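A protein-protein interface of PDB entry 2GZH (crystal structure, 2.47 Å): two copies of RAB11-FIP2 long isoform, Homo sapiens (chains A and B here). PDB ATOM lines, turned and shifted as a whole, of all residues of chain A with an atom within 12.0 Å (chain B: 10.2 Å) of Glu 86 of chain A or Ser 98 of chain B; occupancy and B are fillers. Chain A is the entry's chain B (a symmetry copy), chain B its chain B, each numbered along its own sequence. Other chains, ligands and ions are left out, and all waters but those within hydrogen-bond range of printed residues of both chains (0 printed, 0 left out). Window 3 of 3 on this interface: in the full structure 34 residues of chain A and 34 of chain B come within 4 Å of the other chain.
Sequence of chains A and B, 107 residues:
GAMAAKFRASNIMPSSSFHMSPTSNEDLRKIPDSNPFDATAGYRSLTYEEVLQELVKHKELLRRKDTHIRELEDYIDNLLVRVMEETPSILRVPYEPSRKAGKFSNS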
ATOM      1  N   ASP A  77      23.503  15.589  -9.684  1.00  0.00           N
ATOM      2  CA  ASP A  77      22.531  16.644  -9.822  1.00  0.00           C
ATOM      3  C   ASP A  77      23.025  17.764 -10.714  1.00  0.00           C
ATOM      4  O   ASP A  77      22.275  18.272 -11.546  1.00  0.00           O
ATOM      5  CB  ASP A  77      22.160  17.215  -8.443  1.00  0.00           C
ATOM      6  CG  ASP A  77      21.127  16.345  -7.703  1.00  0.00           C
ATOM      7  OD1 ASP A  77      20.637  15.322  -8.296  1.00  0.00           O
ATOM      8  OD2 ASP A  77      20.822  16.684  -6.513  1.00  0.00           O
ATOM      9  N   ASN A  78      24.274  18.160 -10.542  1.00  0.00           N
ATOM     10  CA  ASN A  78      24.815  19.211 -11.373  1.00  0.00           C
ATOM     11  C   ASN A  78      24.968  18.813 -12.814  1.00  0.00           C
ATOM     12  O   ASN A  78      24.810  19.646 -13.676  1.00  0.00           O
ATOM     13  CB  ASN A  78      26.146  19.728 -10.873  1.00  0.00           C
ATOM     14  CG  ASN A  78      26.048  20.345  -9.483  1.00  0.00           C
ATOM     15  OD1 ASN A  78      26.919  20.113  -8.662  1.00  0.00           O
ATOM     16  ND2 ASN A  78      24.980  21.103  -9.202  1.00  0.00           N
ATOM     17  N   LEU A  79      25.251  17.543 -13.077  1.00  0.00           N
ATOM     18  CA  LEU A  79      25.317  17.106 -14.437  1.00  0.00           C
ATOM     19  C   LEU A  79      23.879  17.034 -15.037  1.00  0.00           C
ATOM     20  O   LEU A  79      23.663  17.408 -16.195  1.00  0.00           O
ATOM     21  CB  LEU A  79      26.023  15.761 -14.500  1.00  0.00           C
ATOM     22  CG  LEU A  79      26.022  15.022 -15.841  1.00  0.00           C
ATOM     23  CD1 LEU A  79      26.860  15.777 -16.922  1.00  0.00           C
ATOM     24  CD2 LEU A  79      26.520  13.559 -15.648  1.00  0.00           C
ATOM     25  N   LEU A  80      22.906  16.571 -14.245  1.00  0.00           N
ATOM     26  CA  LEU A  80      21.530  16.460 -14.758  1.00  0.00           C
ATOM     27  C   LEU A  80      20.920  17.814 -15.146  1.00  0.00           C
ATOM     28  O   LEU A  80      20.226  17.909 -16.142  1.00  0.00           O
ATOM     29  CB  LEU A  80      20.635  15.688 -13.795  1.00  0.00           C
ATOM     30  CG  LEU A  80      20.899  14.181 -13.814  1.00  0.00           C
ATOM     31  CD1 LEU A  80      20.054  13.565 -12.807  1.00  0.00           C
ATOM     32  CD2 LEU A  80      20.621  13.587 -15.176  1.00  0.00           C
ATOM     33  N   VAL A  81      21.197  18.863 -14.389  1.00  0.00           N
ATOM     34  CA  VAL A  81      20.751  20.182 -14.785  1.00  0.00           C
ATOM     35  C   VAL A  81      21.165  20.456 -16.240  1.00  0.00           C
ATOM     36  O   VAL A  81      20.334  20.757 -17.109  1.00  0.00           O
ATOM     37  CB  VAL A  81      21.359  21.262 -13.841  1.00  0.00           C
ATOM     38  CG1 VAL A  81      21.025  22.624 -14.297  1.00  0.00           C
ATOM     39  CG2 VAL A  81      20.819  21.071 -12.440  1.00  0.00           C
ATOM     40  N   ARG A  82      22.455  20.363 -16.510  1.00  0.00           N
ATOM     41  CA  ARG A  82      22.963  20.522 -17.889  1.00  0.00           C
ATOM     42  C   ARG A  82      22.312  19.556 -18.879  1.00  0.00           C
ATOM     43  O   ARG A  82      21.953  19.966 -19.961  1.00  0.00           O
ATOM     44  CB  ARG A  82      24.499  20.430 -17.932  1.00  0.00           C
ATOM     45  CG  ARG A  82      25.150  21.433 -16.967  1.00  0.00           C
ATOM     46  CD  ARG A  82      26.679  21.436 -17.074  1.00  0.00           C
ATOM     47  NE  ARG A  82      27.318  20.420 -16.247  1.00  0.00           N
ATOM     48  CZ  ARG A  82      28.637  20.177 -16.185  1.00  0.00           C
ATOM     49  NH1 ARG A  82      29.502  20.920 -16.909  1.00  0.00           N
ATOM     50  NH2 ARG A  82      29.089  19.180 -15.377  1.00  0.00           N
ATOM     51  N   VAL A  83      22.171  18.283 -18.542  1.00  0.00           N
ATOM     52  CA  VAL A  83      21.553  17.332 -19.473  1.00  0.00           C
ATOM     53  C   VAL A  83      20.115  17.741 -19.799  1.00  0.00           C
ATOM     54  O   VAL A  83      19.676  17.706 -20.952  1.00  0.00           O
ATOM     55  CB  VAL A  83      21.545  15.892 -18.955  1.00  0.00           C
ATOM     56  CG1 VAL A  83      20.770  14.996 -19.929  1.00  0.00           C
ATOM     57  CG2 VAL A  83      22.938  15.389 -18.863  1.00  0.00           C
ATOM     58  N   MET A  84      19.433  18.183 -18.760  1.00  0.00           N
ATOM     59  CA  MET A  84      18.070  18.598 -18.858  1.00  0.00           C
ATOM     60  C   MET A  84      17.864  19.832 -19.722  1.00  0.00           C
ATOM     61  O   MET A  84      16.874  19.917 -20.413  1.00  0.00           O
ATOM     62  CB  MET A  84      17.489  18.816 -17.463  1.00  0.00           C
ATOM     63  CG  MET A  84      17.046  17.489 -16.857  1.00  0.00           C
ATOM     64  SD  MET A  84      16.798  17.586 -14.862  1.00  0.00           S
ATOM     65  CE  MET A  84      18.078  16.598 -14.442  1.00  0.00           C
ATOM     66  N   GLU A  85      18.769  20.789 -19.642  1.00  0.00           N
ATOM     67  CA  GLU A  85      18.598  22.019 -20.370  1.00  0.00           C
ATOM     68  C   GLU A  85      19.080  21.888 -21.802  1.00  0.00           C
ATOM     69  O   GLU A  85      18.716  22.722 -22.601  1.00  0.00           O
ATOM     70  CB  GLU A  85      19.311  23.185 -19.692  1.00  0.00           C
ATOM     71  CG  GLU A  85      18.524  23.789 -18.523  1.00  0.00           C
ATOM     72  CD  GLU A  85      19.407  24.556 -17.510  1.00  0.00           C
ATOM     73  OE1 GLU A  85      20.650  24.746 -17.734  1.00  0.00           O
ATOM     74  OE2 GLU A  85      18.865  24.960 -16.458  1.00  0.00           O
ATOM     75  N   GLU A  86      19.866  20.861 -22.122  1.00  0.00           N
ATOM     76  CA  GLU A  86      20.481  20.772 -23.418  1.00  0.00           C
ATOM     77  C   GLU A  86      19.973  19.620 -24.239  1.00  0.00           C
ATOM     78  O   GLU A  86      19.616  19.824 -25.376  1.00  0.00           O
ATOM     79  CB  GLU A  86      22.005  20.660 -23.312  1.00  0.00           C
ATOM     80  CG  GLU A  86      22.640  21.842 -22.634  1.00  0.00           C
ATOM     81  CD  GLU A  86      23.758  22.454 -23.440  1.00  0.00           C
ATOM     82  OE1 GLU A  86      23.766  22.297 -24.670  1.00  0.00           O
ATOM     83  OE2 GLU A  86      24.637  23.113 -22.847  1.00  0.00           O
ATOM     84  N   THR A  87      19.952  18.413 -23.670  1.00  0.00           N
ATOM     85  CA  THR A  87      19.572  17.201 -24.387  1.00  0.00           C
ATOM     86  C   THR A  87      18.768  16.279 -23.452  1.00  0.00           C
ATOM     87  O   THR A  87      19.195  15.168 -23.149  1.00  0.00           O
ATOM     88  CB  THR A  87      20.833  16.495 -24.938  1.00  0.00           C
ATOM     89  OG1 THR A  87      21.638  17.484 -25.577  1.00  0.00           O
ATOM     90  CG2 THR A  87      20.504  15.427 -25.965  1.00  0.00           C
ATOM     91  N   PRO A  88      17.582  16.731 -23.024  1.00  0.00           N
ATOM     92  CA  PRO A  88      16.789  15.950 -22.068  1.00  0.00           C
ATOM     93  C   PRO A  88      16.423  14.570 -22.575  1.00  0.00           C
ATOM     94  O   PRO A  88      16.121  13.676 -21.776  1.00  0.00           O
ATOM     95  CB  PRO A  88      15.540  16.823 -21.848  1.00  0.00           C
ATOM     96  CG  PRO A  88      15.442  17.673 -23.160  1.00  0.00           C
ATOM     97  CD  PRO A  88      16.907  18.000 -23.389  1.00  0.00           C
ATOM     98  N   SER A  89      16.485  14.374 -23.887  1.00  0.00           N
ATOM     99  CA  SER A  89      16.135  13.091 -24.459  1.00  0.00           C
ATOM    100  C   SER A  89      17.052  11.981 -23.998  1.00  0.00           C
ATOM    101  O   SER A  89      16.673  10.787 -24.070  1.00  0.00           O
ATOM    102  CB  SER A  89      16.121  13.142 -25.997  1.00  0.00           C
ATOM    103  OG  SER A  89      17.386  13.543 -26.525  1.00  0.00           O
ATOM    104  N   ILE A  90      18.262  12.330 -23.547  1.00  0.00           N
ATOM    105  CA  ILE A  90      19.107  11.260 -23.021  1.00  0.00           C
ATOM    106  C   ILE A  90      18.547  10.651 -21.721  1.00  0.00           C
ATOM    107  O   ILE A  90      18.971   9.585 -21.320  1.00  0.00           O
ATOM    108  CB  ILE A  90      20.612  11.615 -22.878  1.00  0.00           C
ATOM    109  CG1 ILE A  90      20.971  11.886 -21.454  1.00  0.00           C
ATOM    110  CG2 ILE A  90      21.159  12.765 -23.839  1.00  0.00           C
ATOM    111  CD1 ILE A  90      22.473  12.025 -21.345  1.00  0.00           C
ATOM    112  N   LEU A  91      17.573  11.312 -21.086  1.00  0.00           N
ATOM    113  CA  LEU A  91      16.984  10.805 -19.849  1.00  0.00           C
ATOM    114  C   LEU A  91      15.757   9.926 -20.075  1.00  0.00           C
ATOM    115  O   LEU A  91      15.241   9.327 -19.129  1.00  0.00           O
ATOM    116  CB  LEU A  91      16.676  11.948 -18.882  1.00  0.00           C
ATOM    117  CG  LEU A  91      17.868  12.853 -18.593  1.00  0.00           C
ATOM    118  CD1 LEU A  91      17.444  14.038 -17.734  1.00  0.00           C
ATOM    119  CD2 LEU A  91      19.056  12.041 -17.950  1.00  0.00           C
ATOM    120  N   ARG A  92      15.332   9.824 -21.337  1.00  0.00           N
ATOM    121  CA  ARG A  92      14.268   8.888 -21.795  1.00  0.00           C
ATOM    122  C   ARG A  92      14.525   7.375 -21.553  1.00  0.00           C
ATOM    123  O   ARG A  92      15.670   6.917 -21.623  1.00  0.00           O
ATOM    124  CB  ARG A  92      13.956   9.191 -23.261  1.00  0.00           C
ATOM    125  CG  ARG A  92      13.085   8.208 -23.955  1.00  0.00           C
ATOM    126  CD  ARG A  92      11.663   8.621 -24.035  1.00  0.00           C
ATOM    127  NE  ARG A  92      11.362   9.206 -25.342  1.00  0.00           N
ATOM    128  CZ  ARG A  92      10.524   8.676 -26.237  1.00  0.00           C
ATOM    129  NH1 ARG A  92       9.894   7.540 -25.983  1.00  0.00           N
ATOM    130  NH2 ARG A  92      10.309   9.285 -27.394  1.00  0.00           N
ATOM    131  N   TYR A  95      16.092   4.422 -23.834  1.00  0.00           N
ATOM    132  CA  TYR A  95      16.997   5.360 -24.470  1.00  0.00           C
ATOM    133  C   TYR A  95      17.091   5.180 -25.979  1.00  0.00           C
ATOM    134  O   TYR A  95      17.653   4.213 -26.470  1.00  0.00           O
ATOM    135  CB  TYR A  95      18.381   5.255 -23.853  1.00  0.00           C
ATOM    136  CG  TYR A  95      19.397   6.123 -24.529  1.00  0.00           C
ATOM    137  CD1 TYR A  95      19.219   7.485 -24.603  1.00  0.00           C
ATOM    138  CD2 TYR A  95      20.529   5.582 -25.098  1.00  0.00           C
ATOM    139  CE1 TYR A  95      20.140   8.286 -25.218  1.00  0.00           C
ATOM    140  CE2 TYR A  95      21.455   6.374 -25.711  1.00  0.00           C
ATOM    141  CZ  TYR A  95      21.256   7.729 -25.771  1.00  0.00           C
ATOM    142  OH  TYR A  95      22.172   8.534 -26.382  1.00  0.00           O
ATOM    143  N   GLU A  96      16.525   6.130 -26.726  1.00  0.00           N
ATOM    144  CA  GLU A  96      16.717   6.250 -28.166  1.00  0.00           C
ATOM    145  C   GLU A  96      17.862   7.202 -28.492  1.00  0.00           C
ATOM    146  O   GLU A  96      17.744   8.442 -28.301  1.00  0.00           O
ATOM    147  CB  GLU A  96      15.428   6.725 -28.839  1.00  0.00           C
ATOM    148  CG  GLU A  96      14.877   8.027 -28.281  1.00  0.00           C
ATOM    149  CD  GLU A  96      13.631   8.492 -29.009  1.00  0.00           C
ATOM    150  OE1 GLU A  96      13.222   7.819 -29.977  1.00  0.00           O
ATOM    151  OE2 GLU A  96      13.063   9.532 -28.614  1.00  0.00           O
ATOM    152  N   SER A  98      20.147   9.695 -30.426  1.00  0.00           N
ATOM    153  CA  SER A  98      19.666  10.696 -31.367  1.00  0.00           C
ATOM    154  C   SER A  98      20.716  11.111 -32.433  1.00  0.00           C
ATOM    155  O   SER A  98      20.337  11.608 -33.507  1.00  0.00           O
ATOM    156  CB  SER A  98      19.114  11.890 -30.581  1.00  0.00           C
ATOM    157  OG  SER A  98      18.864  13.013 -31.403  1.00  0.00           O
ATOM    158  N   VAL B  83      26.073  11.063 -22.614  1.00  0.00           N
ATOM    159  CA  VAL B  83      26.452  12.476 -22.730  1.00  0.00           C
ATOM    160  C   VAL B  83      27.585  12.657 -23.742  1.00  0.00           C
ATOM    161  O   VAL B  83      27.572  13.568 -24.576  1.00  0.00           O
ATOM    162  CB  VAL B  83      26.881  13.102 -21.401  1.00  0.00           C
ATOM    163  CG1 VAL B  83      27.380  14.532 -21.640  1.00  0.00           C
ATOM    164  CG2 VAL B  83      25.719  13.157 -20.480  1.00  0.00           C
ATOM    165  N   GLU B  86      26.462  12.195 -27.446  1.00  0.00           N
ATOM    166  CA  GLU B  86      25.439  13.073 -27.942  1.00  0.00           C
ATOM    167  C   GLU B  86      25.790  14.529 -27.809  1.00  0.00           C
ATOM    168  O   GLU B  86      25.669  15.251 -28.771  1.00  0.00           O
ATOM    169  CB  GLU B  86      24.099  12.830 -27.242  1.00  0.00           C
ATOM    170  CG  GLU B  86      23.574  11.435 -27.436  1.00  0.00           C
ATOM    171  CD  GLU B  86      22.155  11.404 -27.948  1.00  0.00           C
ATOM    172  OE1 GLU B  86      21.724  12.381 -28.578  1.00  0.00           O
ATOM    173  OE2 GLU B  86      21.460  10.389 -27.734  1.00  0.00           O
ATOM    174  N   THR B  87      26.212  14.960 -26.618  1.00  0.00           N
ATOM    175  CA  THR B  87      26.494  16.362 -26.333  1.00  0.00           C
ATOM    176  C   THR B  87      27.722  16.465 -25.409  1.00  0.00           C
ATOM    177  O   THR B  87      27.620  16.946 -24.284  1.00  0.00           O
ATOM    178  CB  THR B  87      25.250  17.035 -25.705  1.00  0.00           C
ATOM    179  OG1 THR B  87      24.119  16.677 -26.498  1.00  0.00           O
ATOM    180  CG2 THR B  87      25.348  18.549 -25.691  1.00  0.00           C
ATOM    181  N   PRO B  88      28.892  16.042 -25.904  1.00  0.00           N
ATOM    182  CA  PRO B  88      30.094  16.031 -25.062  1.00  0.00           C
ATOM    183  C   PRO B  88      30.467  17.398 -24.527  1.00  0.00           C
ATOM    184  O   PRO B  88      31.180  17.496 -23.522  1.00  0.00           O
ATOM    185  CB  PRO B  88      31.179  15.476 -26.004  1.00  0.00           C
ATOM    186  CG  PRO B  88      30.652  15.835 -27.435  1.00  0.00           C
ATOM    187  CD  PRO B  88      29.173  15.536 -27.269  1.00  0.00           C
ATOM    188  N   SER B  89      29.962  18.451 -25.158  1.00  0.00           N
ATOM    189  CA  SER B  89      30.281  19.795 -24.725  1.00  0.00           C
ATOM    190  C   SER B  89      29.788  20.085 -23.325  1.00  0.00           C
ATOM    191  O   SER B  89      30.301  21.018 -22.662  1.00  0.00           O
ATOM    192  CB  SER B  89      29.723  20.850 -25.696  1.00  0.00           C
ATOM    193  OG  SER B  89      28.306  20.744 -25.837  1.00  0.00           O
ATOM    194  N   ILE B  90      28.787  19.330 -22.858  1.00  0.00           N
ATOM    195  CA  ILE B  90      28.377  19.558 -21.474  1.00  0.00           C
ATOM    196  C   ILE B  90      29.463  19.147 -20.461  1.00  0.00           C
ATOM    197  O   ILE B  90      29.393  19.529 -19.309  1.00  0.00           O
ATOM    198  CB  ILE B  90      26.992  18.970 -21.088  1.00  0.00           C
ATOM    199  CG1 ILE B  90      27.140  17.718 -20.287  1.00  0.00           C
ATOM    200  CG2 ILE B  90      25.954  18.771 -22.283  1.00  0.00           C
ATOM    201  CD1 ILE B  90      25.781  17.303 -19.771  1.00  0.00           C
ATOM    202  N   LEU B  91      30.482  18.400 -20.901  1.00  0.00           N
ATOM    203  CA  LEU B  91      31.555  17.969 -20.009  1.00  0.00           C
ATOM    204  C   LEU B  91      32.740  18.931 -19.972  1.00  0.00           C
ATOM    205  O   LEU B  91      33.655  18.757 -19.165  1.00  0.00           O
ATOM    206  CB  LEU B  91      32.008  16.547 -20.346  1.00  0.00           C
ATOM    207  CG  LEU B  91      30.875  15.529 -20.375  1.00  0.00           C
ATOM    208  CD1 LEU B  91      31.386  14.174 -20.850  1.00  0.00           C
ATOM    209  CD2 LEU B  91      30.152  15.441 -18.978  1.00  0.00           C
ATOM    210  N   ARG B  92      32.685  19.963 -20.818  1.00  0.00           N
ATOM    211  CA  ARG B  92      33.644  21.102 -20.822  1.00  0.00           C
ATOM    212  C   ARG B  92      33.740  21.930 -19.511  1.00  0.00           C
ATOM    213  O   ARG B  92      32.739  22.110 -18.811  1.00  0.00           O
ATOM    214  CB  ARG B  92      33.345  21.982 -22.037  1.00  0.00           C
ATOM    215  CG  ARG B  92      34.048  23.289 -22.080  1.00  0.00           C
ATOM    216  CD  ARG B  92      35.256  23.291 -22.941  1.00  0.00           C
ATOM    217  NE  ARG B  92      34.960  23.862 -24.254  1.00  0.00           N
ATOM    218  CZ  ARG B  92      35.487  24.995 -24.727  1.00  0.00           C
ATOM    219  NH1 ARG B  92      36.339  25.698 -23.999  1.00  0.00           N
ATOM    220  NH2 ARG B  92      35.162  25.429 -25.936  1.00  0.00           N
ATOM    221  N   PRO B  94      35.553  25.450 -18.664  1.00  0.00           N
ATOM    222  CA  PRO B  94      34.317  25.692 -17.938  1.00  0.00           C
ATOM    223  C   PRO B  94      33.107  25.514 -18.838  1.00  0.00           C
ATOM    224  O   PRO B  94      33.229  25.551 -20.052  1.00  0.00           O
ATOM    225  CB  PRO B  94      34.461  27.143 -17.531  1.00  0.00           C
ATOM    226  CG  PRO B  94      35.206  27.741 -18.639  1.00  0.00           C
ATOM    227  CD  PRO B  94      36.150  26.704 -19.142  1.00  0.00           C
ATOM    228  N   TYR B  95      31.946  25.324 -18.228  1.00  0.00           N
ATOM    229  CA  TYR B  95      30.732  24.982 -18.946  1.00  0.00           C
ATOM    230  C   TYR B  95      30.124  26.159 -19.697  1.00  0.00           C
ATOM    231  O   TYR B  95      29.585  27.081 -19.103  1.00  0.00           O
ATOM    232  CB  TYR B  95      29.706  24.394 -17.993  1.00  0.00           C
ATOM    233  CG  TYR B  95      28.388  24.112 -18.644  1.00  0.00           C
ATOM    234  CD1 TYR B  95      28.304  23.257 -19.718  1.00  0.00           C
ATOM    235  CD2 TYR B  95      27.230  24.705 -18.191  1.00  0.00           C
ATOM    236  CE1 TYR B  95      27.107  22.992 -20.320  1.00  0.00           C
ATOM    237  CE2 TYR B  95      26.029  24.444 -18.784  1.00  0.00           C
ATOM    238  CZ  TYR B  95      25.971  23.587 -19.852  1.00  0.00           C
ATOM    239  OH  TYR B  95      24.777  23.318 -20.456  1.00  0.00           O
ATOM    240  N   GLU B  96      30.217  26.125 -21.027  1.00  0.00           N
ATOM    241  CA  GLU B  96      29.495  27.031 -21.913  1.00  0.00           C
ATOM    242  C   GLU B  96      28.172  26.422 -22.366  1.00  0.00           C
ATOM    243  O   GLU B  96      28.151  25.452 -23.170  1.00  0.00           O
ATOM    244  CB  GLU B  96      30.354  27.388 -23.128  1.00  0.00           C
ATOM    245  CG  GLU B  96      30.853  26.186 -23.912  1.00  0.00           C
ATOM    246  CD  GLU B  96      31.654  26.582 -25.137  1.00  0.00           C
ATOM    247  OE1 GLU B  96      31.784  27.796 -25.396  1.00  0.00           O
ATOM    248  OE2 GLU B  96      32.152  25.678 -25.842  1.00  0.00           O
ATOM    249  N   PRO B  97      27.027  26.935 -21.832  1.00  0.00           N
ATOM    250  CA  PRO B  97      25.687  26.488 -22.268  1.00  0.00           C
ATOM    251  C   PRO B  97      25.484  26.711 -23.775  1.00  0.00           C
ATOM    252  O   PRO B  97      25.805  27.782 -24.304  1.00  0.00           O
ATOM    253  CB  PRO B  97      24.719  27.365 -21.447  1.00  0.00           C
ATOM    254  CG  PRO B  97      25.561  28.501 -20.920  1.00  0.00           C
ATOM    255  CD  PRO B  97      26.952  27.959 -20.771  1.00  0.00           C
ATOM    256  N   SER B  98      24.969  25.707 -24.463  1.00  0.00           N
ATOM    257  CA  SER B  98      24.905  25.762 -25.917  1.00  0.00           C
ATOM    258  C   SER B  98      23.485  26.061 -26.471  1.00  0.00           C
ATOM    259  O   SER B  98      23.360  26.540 -27.611  1.00  0.00           O
ATOM    260  CB  SER B  98      25.506  24.473 -26.488  1.00  0.00           C
ATOM    261  OG  SER B  98      25.253  24.323 -27.871  1.00  0.00           O
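OH of Tyr 95 of chain A lies within hydrogen-bond range of OE2 of Glu 86 of chain B (2.4 Å).
N of Ser 98 of chain A sits at hydrogen-bond distance from OE2 of Glu 86 of chain B (3.1 Å).
The side-chain hydroxyl (OG1) of Thr 87 of chain B sits at hydrogen-bond distance from the side-chain hydroxyl (OG1) of Thr 87 of chain A.
The backbone carbonyl oxygen of Ile 90 of chain B is in hydrogen-bond range of the guanidinium group of Arg 82 of chain A.
The side-chain carboxylate (OE2) of Glu 86 of chain A sits at hydrogen-bond distance from the side-chain hydroxyl (OH) of Tyr 95 of chain B (2.4 Å).
The backbone NH (N) of Ser 98 of chain B lies within hydrogen-bond range of the side-chain carboxylate (OE2) of Glu 86 of chain A (3.1 Å).
NH2 of Arg 92 of chain B lies within salt-bridge range of OE2 of Glu 96 of chain B, at 3.0 Å.
Ile 90 of chain B touches Leu 79 of chain A.
Leu 79 of chain A touches Leu 91 of chain B.
Arg 92 of chain B touches Arg 82 of chain A (O to NH1, 3.9 Å).
Arg 82 of chain A touches Tyr 95 of chain B.
Val 83 of chain B touches Val 83 of chain A (CG2 to CG2, 3.9 Å).
Ile 90 of chain B touches Val 83 of chain A (CD1 to CG2, 3.5 Å).
Glu 86 of chain A touches Pro 97 of chain B.
Ile 90 of chain A touches Val 83 of chain B (CD1 to CG2, 3.5 Å).
Printed residues of chain B within 4 Å of Val 83 of chain A: Val 83 (3.9 Å) and Ile 90 (3.5 Å).
Of chain B, only Tyr 95 (2.4 Å), Pro 97 (3.6 Å) and Ser 98 (3.1 Å) come within 4 Å of Glu 86 of chain A.
Thr 87 of chain A touches one residue of chain B.
Printed residues of chain B within 4 Å of Ile 90 of chain A: Val 83 (3.5 Å).
Printed residues of chain B within 4 Å of Ser 98 of chain A: Glu 86.
Of the printed residues of chain A, Glu 86 of chain B touches Tyr 95 (2.4 Å) and Ser 98 (3.1 Å).
Thr 87 of chain B touches just one residue of chain A: Thr 87 (2.8 Å).
Pro 88 of chain B touches none of the printed residues of chain A.
No residue of chain A comes within 4 Å of Ser 89 of chain B.
Of chain A, only Leu 79, Arg 82 and Val 83 come within 4 Å of Ile 90 of chain B.
Printed residues of chain A within 4 Å of Tyr 95 of chain B: Arg 82 and Glu 86.
No residue of chain A comes within 4 Å of Glu 96 of chain B.
The nearest residue of chain B that does not touch Glu 86 of chain A is Thr 87 of chain B (4.2 Å).
The nearest printed residue of chain B that does not touch Val 83 of chain A is Tyr 95 of chain B (6.0 Å).
Of the 19 printed residues of chain A, 8 touch a printed residue of chain B.
Hydrophobic or aromatic side chains of chain A within 4 Å of the printed part of chain B: Leu 79, Val 83, Ile 90 and Tyr 95.
Along chain A the printed residues that touch a printed residue of chain B span positions 79 to 98.
Val 83 of chain A touches its own counterpart, Val 83 of chain B.
Val 83 of chain A touches Ile 90 of chain B, and with the chains exchanged Ile 90 of chain A touches Val 83 of chain B.
Glu 86 of chain A touches Tyr 95 of chain B, and with the chains exchanged Tyr 95 of chain A touches Glu 86 of chain B.
Glu 86 of chain A touches Ser 98 of chain B, and with the chains exchanged Ser 98 of chain A touches Glu 86 of chain B.
11 positions are printed for both chains.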
